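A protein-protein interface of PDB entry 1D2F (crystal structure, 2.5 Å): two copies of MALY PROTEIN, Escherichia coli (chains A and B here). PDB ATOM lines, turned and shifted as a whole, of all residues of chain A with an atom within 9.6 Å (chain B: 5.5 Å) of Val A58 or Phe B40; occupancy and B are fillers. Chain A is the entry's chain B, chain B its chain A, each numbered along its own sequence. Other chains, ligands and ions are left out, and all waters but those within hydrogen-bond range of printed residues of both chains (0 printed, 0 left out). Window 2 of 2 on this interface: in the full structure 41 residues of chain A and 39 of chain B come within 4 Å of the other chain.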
ATOM      1  N   GLN A  52      20.419  37.601  23.557  1.00  0.00           N
ATOM      2  CA  GLN A  52      21.729  37.181  24.032  1.00  0.00           C
ATOM      3  C   GLN A  52      22.194  35.918  23.307  1.00  0.00           C
ATOM      4  O   GLN A  52      23.331  35.841  22.853  1.00  0.00           O
ATOM      5  CB  GLN A  52      21.663  36.927  25.532  1.00  0.00           C
ATOM      6  CG  GLN A  52      23.006  36.795  26.203  1.00  0.00           C
ATOM      7  CD  GLN A  52      22.873  36.239  27.607  1.00  0.00           C
ATOM      8  OE1 GLN A  52      22.049  36.716  28.398  1.00  0.00           O
ATOM      9  NE2 GLN A  52      23.683  35.225  27.929  1.00  0.00           N
ATOM     10  N   ARG A  53      21.309  34.932  23.213  1.00  0.00           N
ATOM     11  CA  ARG A  53      21.616  33.673  22.537  1.00  0.00           C
ATOM     12  C   ARG A  53      21.848  33.991  21.067  1.00  0.00           C
ATOM     13  O   ARG A  53      22.595  33.304  20.372  1.00  0.00           O
ATOM     14  CB  ARG A  53      20.436  32.698  22.696  1.00  0.00           C
ATOM     15  CG  ARG A  53      20.589  31.325  22.042  1.00  0.00           C
ATOM     16  CD  ARG A  53      21.867  30.632  22.471  1.00  0.00           C
ATOM     17  NE  ARG A  53      22.870  30.744  21.420  1.00  0.00           N
ATOM     18  CZ  ARG A  53      22.868  30.019  20.304  1.00  0.00           C
ATOM     19  NH1 ARG A  53      21.923  29.115  20.097  1.00  0.00           N
ATOM     20  NH2 ARG A  53      23.787  30.227  19.375  1.00  0.00           N
ATOM     21  N   LEU A  54      21.212  35.061  20.611  1.00  0.00           N
ATOM     22  CA  LEU A  54      21.327  35.494  19.228  1.00  0.00           C
ATOM     23  C   LEU A  54      22.740  36.000  18.936  1.00  0.00           C
ATOM     24  O   LEU A  54      23.348  35.636  17.929  1.00  0.00           O
ATOM     25  CB  LEU A  54      20.306  36.602  18.960  1.00  0.00           C
ATOM     26  CG  LEU A  54      19.662  36.653  17.575  1.00  0.00           C
ATOM     27  CD1 LEU A  54      20.702  37.011  16.531  1.00  0.00           C
ATOM     28  CD2 LEU A  54      19.019  35.301  17.273  1.00  0.00           C
ATOM     29  N   MET A  55      23.265  36.827  19.835  1.00  0.00           N
ATOM     30  CA  MET A  55      24.596  37.392  19.663  1.00  0.00           C
ATOM     31  C   MET A  55      25.724  36.374  19.707  1.00  0.00           C
ATOM     32  O   MET A  55      26.874  36.718  19.447  1.00  0.00           O
ATOM     33  CB  MET A  55      24.843  38.496  20.695  1.00  0.00           C
ATOM     34  CG  MET A  55      23.897  39.680  20.538  1.00  0.00           C
ATOM     35  SD  MET A  55      23.503  39.999  18.793  1.00  0.00           S
ATOM     36  CE  MET A  55      24.706  41.298  18.363  1.00  0.00           C
ATOM     37  N   HIS A  56      25.414  35.125  20.035  1.00  0.00           N
ATOM     38  CA  HIS A  56      26.457  34.109  20.059  1.00  0.00           C
ATOM     39  C   HIS A  56      26.764  33.688  18.617  1.00  0.00           C
ATOM     40  O   HIS A  56      27.796  33.083  18.342  1.00  0.00           O
ATOM     41  CB  HIS A  56      26.029  32.901  20.887  1.00  0.00           C
ATOM     42  CG  HIS A  56      27.043  31.803  20.901  1.00  0.00           C
ATOM     43  ND1 HIS A  56      26.991  30.732  20.035  1.00  0.00           N
ATOM     44  CD2 HIS A  56      28.163  31.635  21.644  1.00  0.00           C
ATOM     45  CE1 HIS A  56      28.035  29.950  20.243  1.00  0.00           C
ATOM     46  NE2 HIS A  56      28.761  30.475  21.215  1.00  0.00           N
ATOM     47  N   GLY A  57      25.842  34.002  17.711  1.00  0.00           N
ATOM     48  CA  GLY A  57      26.030  33.716  16.298  1.00  0.00           C
ATOM     49  C   GLY A  57      25.992  32.301  15.756  1.00  0.00           C
ATOM     50  O   GLY A  57      25.497  32.091  14.648  1.00  0.00           O
ATOM     51  N   VAL A  58      26.512  31.332  16.502  1.00  0.00           N
ATOM     52  CA  VAL A  58      26.528  29.951  16.031  1.00  0.00           C
ATOM     53  C   VAL A  58      25.194  29.252  16.239  1.00  0.00           C
ATOM     54  O   VAL A  58      24.629  29.298  17.323  1.00  0.00           O
ATOM     55  CB  VAL A  58      27.591  29.145  16.759  1.00  0.00           C
ATOM     56  CG1 VAL A  58      27.777  27.795  16.070  1.00  0.00           C
ATOM     57  CG2 VAL A  58      28.881  29.929  16.808  1.00  0.00           C
ATOM     58  N   PHE A  59      24.697  28.589  15.200  1.00  0.00           N
ATOM     59  CA  PHE A  59      23.419  27.891  15.287  1.00  0.00           C
ATOM     60  C   PHE A  59      23.500  26.436  14.853  1.00  0.00           C
ATOM     61  O   PHE A  59      22.644  25.941  14.118  1.00  0.00           O
ATOM     62  CB  PHE A  59      22.368  28.624  14.461  1.00  0.00           C
ATOM     63  CG  PHE A  59      22.004  29.966  15.016  1.00  0.00           C
ATOM     64  CD1 PHE A  59      22.561  31.126  14.495  1.00  0.00           C
ATOM     65  CD2 PHE A  59      21.109  30.070  16.080  1.00  0.00           C
ATOM     66  CE1 PHE A  59      22.234  32.377  15.022  1.00  0.00           C
ATOM     67  CE2 PHE A  59      20.774  31.314  16.620  1.00  0.00           C
ATOM     68  CZ  PHE A  59      21.341  32.473  16.086  1.00  0.00           C
ATOM     69  N   GLY A  60      24.540  25.757  15.320  1.00  0.00           N
ATOM     70  CA  GLY A  60      24.723  24.360  14.991  1.00  0.00           C
ATOM     71  C   GLY A  60      23.779  23.491  15.791  1.00  0.00           C
ATOM     72  O   GLY A  60      23.004  23.994  16.604  1.00  0.00           O
ATOM     73  N   TYR A  61      23.846  22.183  15.569  1.00  0.00           N
ATOM     74  CA  TYR A  61      22.984  21.236  16.260  1.00  0.00           C
ATOM     75  C   TYR A  61      23.073  21.336  17.785  1.00  0.00           C
ATOM     76  O   TYR A  61      24.163  21.416  18.362  1.00  0.00           O
ATOM     77  CB  TYR A  61      23.316  19.806  15.814  1.00  0.00           C
ATOM     78  CG  TYR A  61      22.884  19.471  14.395  1.00  0.00           C
ATOM     79  CD1 TYR A  61      21.540  19.535  14.024  1.00  0.00           C
ATOM     80  CD2 TYR A  61      23.819  19.077  13.426  1.00  0.00           C
ATOM     81  CE1 TYR A  61      21.135  19.214  12.732  1.00  0.00           C
ATOM     82  CE2 TYR A  61      23.421  18.754  12.126  1.00  0.00           C
ATOM     83  CZ  TYR A  61      22.078  18.826  11.787  1.00  0.00           C
ATOM     84  OH  TYR A  61      21.659  18.511  10.510  1.00  0.00           O
ATOM     85  N   SER A  62      21.912  21.326  18.435  1.00  0.00           N
ATOM     86  CA  SER A  62      21.841  21.401  19.892  1.00  0.00           C
ATOM     87  C   SER A  62      20.980  20.259  20.420  1.00  0.00           C
ATOM     88  O   SER A  62      20.103  19.757  19.719  1.00  0.00           O
ATOM     89  CB  SER A  62      21.241  22.740  20.332  1.00  0.00           C
ATOM     90  OG  SER A  62      21.991  23.832  19.826  1.00  0.00           O
ATOM     91  N   VAL A 271      16.809  25.660  19.140  1.00  0.00           N
ATOM     92  CA  VAL A 271      17.528  26.124  20.313  1.00  0.00           C
ATOM     93  C   VAL A 271      16.850  27.346  20.939  1.00  0.00           C
ATOM     94  O   VAL A 271      16.934  27.547  22.152  1.00  0.00           O
ATOM     95  CB  VAL A 271      19.009  26.463  19.947  1.00  0.00           C
ATOM     96  CG1 VAL A 271      19.081  27.752  19.148  1.00  0.00           C
ATOM     97  CG2 VAL A 271      19.844  26.556  21.199  1.00  0.00           C
ATOM     98  N   LEU A 272      16.181  28.162  20.125  1.00  0.00           N
ATOM     99  CA  LEU A 272      15.518  29.347  20.661  1.00  0.00           C
ATOM    100  C   LEU A 272      14.256  29.020  21.448  1.00  0.00           C
ATOM    101  O   LEU A 272      13.894  29.756  22.362  1.00  0.00           O
ATOM    102  CB  LEU A 272      15.209  30.345  19.548  1.00  0.00           C
ATOM    103  CG  LEU A 272      16.475  30.944  18.922  1.00  0.00           C
ATOM    104  CD1 LEU A 272      16.106  31.902  17.798  1.00  0.00           C
ATOM    105  CD2 LEU A 272      17.270  31.670  19.991  1.00  0.00           C
ATOM    106  N   THR A 275      15.589  28.170  24.825  1.00  0.00           N
ATOM    107  CA  THR A 275      16.006  29.398  25.496  1.00  0.00           C
ATOM    108  C   THR A 275      14.825  30.203  26.018  1.00  0.00           C
ATOM    109  O   THR A 275      14.873  30.714  27.134  1.00  0.00           O
ATOM    110  CB  THR A 275      16.824  30.275  24.558  1.00  0.00           C
ATOM    111  OG1 THR A 275      18.034  29.587  24.212  1.00  0.00           O
ATOM    112  CG2 THR A 275      17.154  31.600  25.217  1.00  0.00           C
ATOM    113  N   MET B  38      28.921  22.768  10.959  1.00  0.00           N
ATOM    114  CA  MET B  38      30.191  23.499  10.939  1.00  0.00           C
ATOM    115  C   MET B  38      30.462  24.199  12.275  1.00  0.00           C
ATOM    116  O   MET B  38      29.602  24.225  13.152  1.00  0.00           O
ATOM    117  CB  MET B  38      30.183  24.541   9.816  1.00  0.00           C
ATOM    118  CG  MET B  38      29.885  23.982   8.424  1.00  0.00           C
ATOM    119  SD  MET B  38      30.166  25.175   7.077  1.00  0.00           S
ATOM    120  CE  MET B  38      28.496  25.635   6.620  1.00  0.00           C
ATOM    121  N   ASP B  39      31.656  24.764  12.422  1.00  0.00           N
ATOM    122  CA  ASP B  39      32.028  25.473  13.643  1.00  0.00           C
ATOM    123  C   ASP B  39      31.927  26.979  13.448  1.00  0.00           C
ATOM    124  O   ASP B  39      32.324  27.745  14.324  1.00  0.00           O
ATOM    125  CB  ASP B  39      33.475  25.167  14.047  1.00  0.00           C
ATOM    126  CG  ASP B  39      33.683  23.740  14.496  1.00  0.00           C
ATOM    127  OD1 ASP B  39      32.693  22.984  14.591  1.00  0.00           O
ATOM    128  OD2 ASP B  39      34.851  23.379  14.764  1.00  0.00           O
ATOM    129  N   PHE B  40      31.413  27.414  12.307  1.00  0.00           N
ATOM    130  CA  PHE B  40      31.336  28.846  12.044  1.00  0.00           C
ATOM    131  C   PHE B  40      30.031  29.489  12.469  1.00  0.00           C
ATOM    132  O   PHE B  40      29.007  28.822  12.608  1.00  0.00           O
ATOM    133  CB  PHE B  40      31.554  29.127  10.554  1.00  0.00           C
ATOM    134  CG  PHE B  40      32.780  28.468   9.984  1.00  0.00           C
ATOM    135  CD1 PHE B  40      32.666  27.514   8.975  1.00  0.00           C
ATOM    136  CD2 PHE B  40      34.048  28.800  10.450  1.00  0.00           C
ATOM    137  CE1 PHE B  40      33.793  26.900   8.441  1.00  0.00           C
ATOM    138  CE2 PHE B  40      35.186  28.188   9.920  1.00  0.00           C
ATOM    139  CZ  PHE B  40      35.055  27.237   8.914  1.00  0.00           C
ATOM    140  N   ALA B  41      30.085  30.799  12.676  1.00  0.00           N
ATOM    141  CA  ALA B  41      28.912  31.565  13.044  1.00  0.00           C
ATOM    142  C   ALA B  41      28.248  31.868  11.714  1.00  0.00           C
ATOM    143  O   ALA B  41      28.936  32.060  10.722  1.00  0.00           O
ATOM    144  CB  ALA B  41      29.322  32.851  13.735  1.00  0.00           C
ATOM    145  N   THR B  42      26.925  31.915  11.679  1.00  0.00           N
ATOM    146  CA  THR B  42      26.229  32.181  10.428  1.00  0.00           C
ATOM    147  C   THR B  42      26.537  33.566   9.895  1.00  0.00           C
ATOM    148  O   THR B  42      27.236  34.353  10.530  1.00  0.00           O
ATOM    149  CB  THR B  42      24.708  32.071  10.592  1.00  0.00           C
ATOM    150  OG1 THR B  42      24.404  30.938  11.411  1.00  0.00           O
ATOM    151  CG2 THR B  42      24.035  31.892   9.234  1.00  0.00           C
ATOM    152  N   ASN B 236      24.728  27.044   8.149  1.00  0.00           N
ATOM    153  CA  ASN B 236      24.918  26.504   9.484  1.00  0.00           C
ATOM    154  C   ASN B 236      23.894  27.030  10.486  1.00  0.00           C
ATOM    155  O   ASN B 236      24.251  27.628  11.501  1.00  0.00           O
ATOM    156  CB  ASN B 236      26.341  26.804   9.961  1.00  0.00           C
ATOM    157  CG  ASN B 236      26.796  25.859  11.046  1.00  0.00           C
ATOM    158  OD1 ASN B 236      26.446  24.677  11.039  1.00  0.00           O
ATOM    159  ND2 ASN B 236      27.597  26.365  11.979  1.00  0.00           N
ATOM    160  N   TRP B 287      28.521  36.291   1.622  1.00  0.00           N
ATOM    161  CA  TRP B 287      29.055  35.519   2.730  1.00  0.00           C
ATOM    162  C   TRP B 287      29.256  34.077   2.295  1.00  0.00           C
ATOM    163  O   TRP B 287      30.264  33.458   2.610  1.00  0.00           O
ATOM    164  CB  TRP B 287      28.095  35.555   3.915  1.00  0.00           C
ATOM    165  CG  TRP B 287      28.592  34.806   5.117  1.00  0.00           C
ATOM    166  CD1 TRP B 287      29.424  35.278   6.098  1.00  0.00           C
ATOM    167  CD2 TRP B 287      28.274  33.457   5.477  1.00  0.00           C
ATOM    168  NE1 TRP B 287      29.637  34.304   7.049  1.00  0.00           N
ATOM    169  CE2 TRP B 287      28.942  33.178   6.693  1.00  0.00           C
ATOM    170  CE3 TRP B 287      27.488  32.456   4.891  1.00  0.00           C
ATOM    171  CZ2 TRP B 287      28.845  31.939   7.337  1.00  0.00           C
ATOM    172  CZ3 TRP B 287      27.391  31.223   5.531  1.00  0.00           C
ATOM    173  CH2 TRP B 287      28.067  30.977   6.746  1.00  0.00           C
ATOM    174  N   LEU B 291      32.760  31.808   2.096  1.00  0.00           N
ATOM    175  CA  LEU B 291      32.846  30.528   2.790  1.00  0.00           C
ATOM    176  C   LEU B 291      33.263  29.427   1.820  1.00  0.00           C
ATOM    177  O   LEU B 291      34.130  28.618   2.131  1.00  0.00           O
ATOM    178  CB  LEU B 291      31.499  30.180   3.443  1.00  0.00           C
ATOM    179  CG  LEU B 291      31.413  28.838   4.170  1.00  0.00           C
ATOM    180  CD1 LEU B 291      32.540  28.742   5.189  1.00  0.00           C
ATOM    181  CD2 LEU B 291      30.054  28.695   4.848  1.00  0.00           C
ATOM    182  N   TYR B 294      36.986  29.536   1.316  1.00  0.00           N
ATOM    183  CA  TYR B 294      37.704  29.114   2.508  1.00  0.00           C
ATOM    184  C   TYR B 294      37.629  27.607   2.687  1.00  0.00           C
ATOM    185  O   TYR B 294      38.625  26.972   3.036  1.00  0.00           O
ATOM    186  CB  TYR B 294      37.127  29.807   3.743  1.00  0.00           C
ATOM    187  CG  TYR B 294      37.961  29.626   4.993  1.00  0.00           C
ATOM    188  CD1 TYR B 294      39.004  30.499   5.288  1.00  0.00           C
ATOM    189  CD2 TYR B 294      37.716  28.574   5.875  1.00  0.00           C
ATOM    190  CE1 TYR B 294      39.782  30.326   6.432  1.00  0.00           C
ATOM    191  CE2 TYR B 294      38.490  28.396   7.016  1.00  0.00           C
ATOM    192  CZ  TYR B 294      39.519  29.275   7.287  1.00  0.00           C
ATOM    193  OH  TYR B 294      40.285  29.096   8.414  1.00  0.00           O
ATOM    194  N   LEU B 295      36.448  27.041   2.457  1.00  0.00           N
ATOM    195  CA  LEU B 295      36.250  25.599   2.606  1.00  0.00           C
ATOM    196  C   LEU B 295      37.013  24.815   1.538  1.00  0.00           C
ATOM    197  O   LEU B 295      37.659  23.803   1.836  1.00  0.00           O
ATOM    198  CB  LEU B 295      34.758  25.248   2.534  1.00  0.00           C
ATOM    199  CG  LEU B 295      33.887  25.610   3.738  1.00  0.00           C
ATOM    200  CD1 LEU B 295      32.461  25.182   3.463  1.00  0.00           C
ATOM    201  CD2 LEU B 295      34.408  24.924   4.986  1.00  0.00           C
ATOM    202  N   ALA B 368      35.629  19.246   7.373  1.00  0.00           N
ATOM    203  CA  ALA B 368      36.502  20.374   7.081  1.00  0.00           C
ATOM    204  C   ALA B 368      35.814  21.711   7.286  1.00  0.00           C
ATOM    205  O   ALA B 368      36.366  22.758   6.959  1.00  0.00           O
ATOM    206  CB  ALA B 368      37.027  20.267   5.651  1.00  0.00           C
ATOM    207  N   GLY B 369      34.602  21.675   7.821  1.00  0.00           N
ATOM    208  CA  GLY B 369      33.880  22.911   8.068  1.00  0.00           C
ATOM    209  C   GLY B 369      34.289  23.490   9.408  1.00  0.00           C
ATOM    210  O   GLY B 369      33.527  23.454  10.379  1.00  0.00           O
ATOM    211  N   CYS B 370      35.500  24.029   9.461  1.00  0.00           N
ATOM    212  CA  CYS B 370      36.019  24.596  10.691  1.00  0.00           C
ATOM    213  C   CYS B 370      37.215  25.486  10.389  1.00  0.00           C
ATOM    214  O   CYS B 370      37.702  25.526   9.259  1.00  0.00           O
ATOM    215  CB  CYS B 370      36.458  23.466  11.618  1.00  0.00           C
ATOM    216  SG  CYS B 370      37.778  22.444  10.918  1.00  0.00           S
ATOM    217  N   PRO B 371      37.704  26.220  11.397  1.00  0.00           N
ATOM    218  CA  PRO B 371      38.861  27.095  11.180  1.00  0.00           C
ATOM    219  C   PRO B 371      40.064  26.221  10.826  1.00  0.00           C
ATOM    220  O   PRO B 371      40.197  25.107  11.344  1.00  0.00           O
ATOM    221  CB  PRO B 371      39.031  27.776  12.531  1.00  0.00           C
ATOM    222  CG  PRO B 371      37.636  27.772  13.092  1.00  0.00           C
ATOM    223  CD  PRO B 371      37.164  26.392  12.755  1.00  0.00           C
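Printed residues of chain B within 4 Å of Gly A57: Ala B41 (3.8 Å) and Thr B42 (3.3 Å).
Printed residues of chain B within 4 Å of Val A58: Phe B40 (3.8 Å).
Of the printed residues of chain B, Phe A59 touches Thr B42 (3.6 Å) and Asn B236 (3.5 Å).
Printed residues of chain A within 4 Å of Phe B40: Val A58 (3.8 Å).
Ala B41 touches one residue of chain A.
Of the printed residues of chain A, Thr B42 touches Gly A57 (3.3 Å) and Phe A59 (3.6 Å).
Of the printed residues of chain A, Asn B236 touches Phe A59 (3.5 Å).
No residue of chain A comes within 4 Å of Gly B369.
The nearest residue of chain B that does not touch Val A58 is Ala B41 (4.1 Å).
The nearest residue of chain A that does not touch Phe B40 is Phe A59 (5.0 Å).
The nearest printed residue of chain A that does not touch Thr B42 is Val A58 (4.8 Å).
Among the printed residues, no Asp or Glu carboxylate lies within 4 Å of a Lys or Arg side-chain nitrogen of the other chain.
The backbone NH (N) of Thr B42 sits at hydrogen-bond distance from the backbone carbonyl oxygen (O) of Gly A57 (3.3 Å).
No position is printed for both chains.
Of the 5 pairs that touch across the chains among the printed residues, none has its exchanged pair printed and touching as well.
The backbone NH of Met B38 lies within hydrogen-bond range of the side-chain amide oxygen of Asn B236 (3.1 Å).
The backbone carbonyl oxygen (O) of Phe B40 is in hydrogen-bond range of the side-chain amide nitrogen (ND2) of Asn B236, 2.9 Å away.
The side-chain hydroxyl of Thr B42 lies within hydrogen-bond range of the backbone carbonyl oxygen of Asn B236 (3.3 Å).
The guanidinium group of Arg A53 sits at hydrogen-bond distance from the backbone carbonyl oxygen of Val A58 (2.4 Å).
Among the printed residues, pairs that only touch across the chains: Gly A57 with Ala B41 (3.8 Å), Val A58 with Phe B40 (3.8 Å), Phe A59 with Thr B42 (3.6 Å) and Phe A59 with Asn B236 (3.5 Å).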
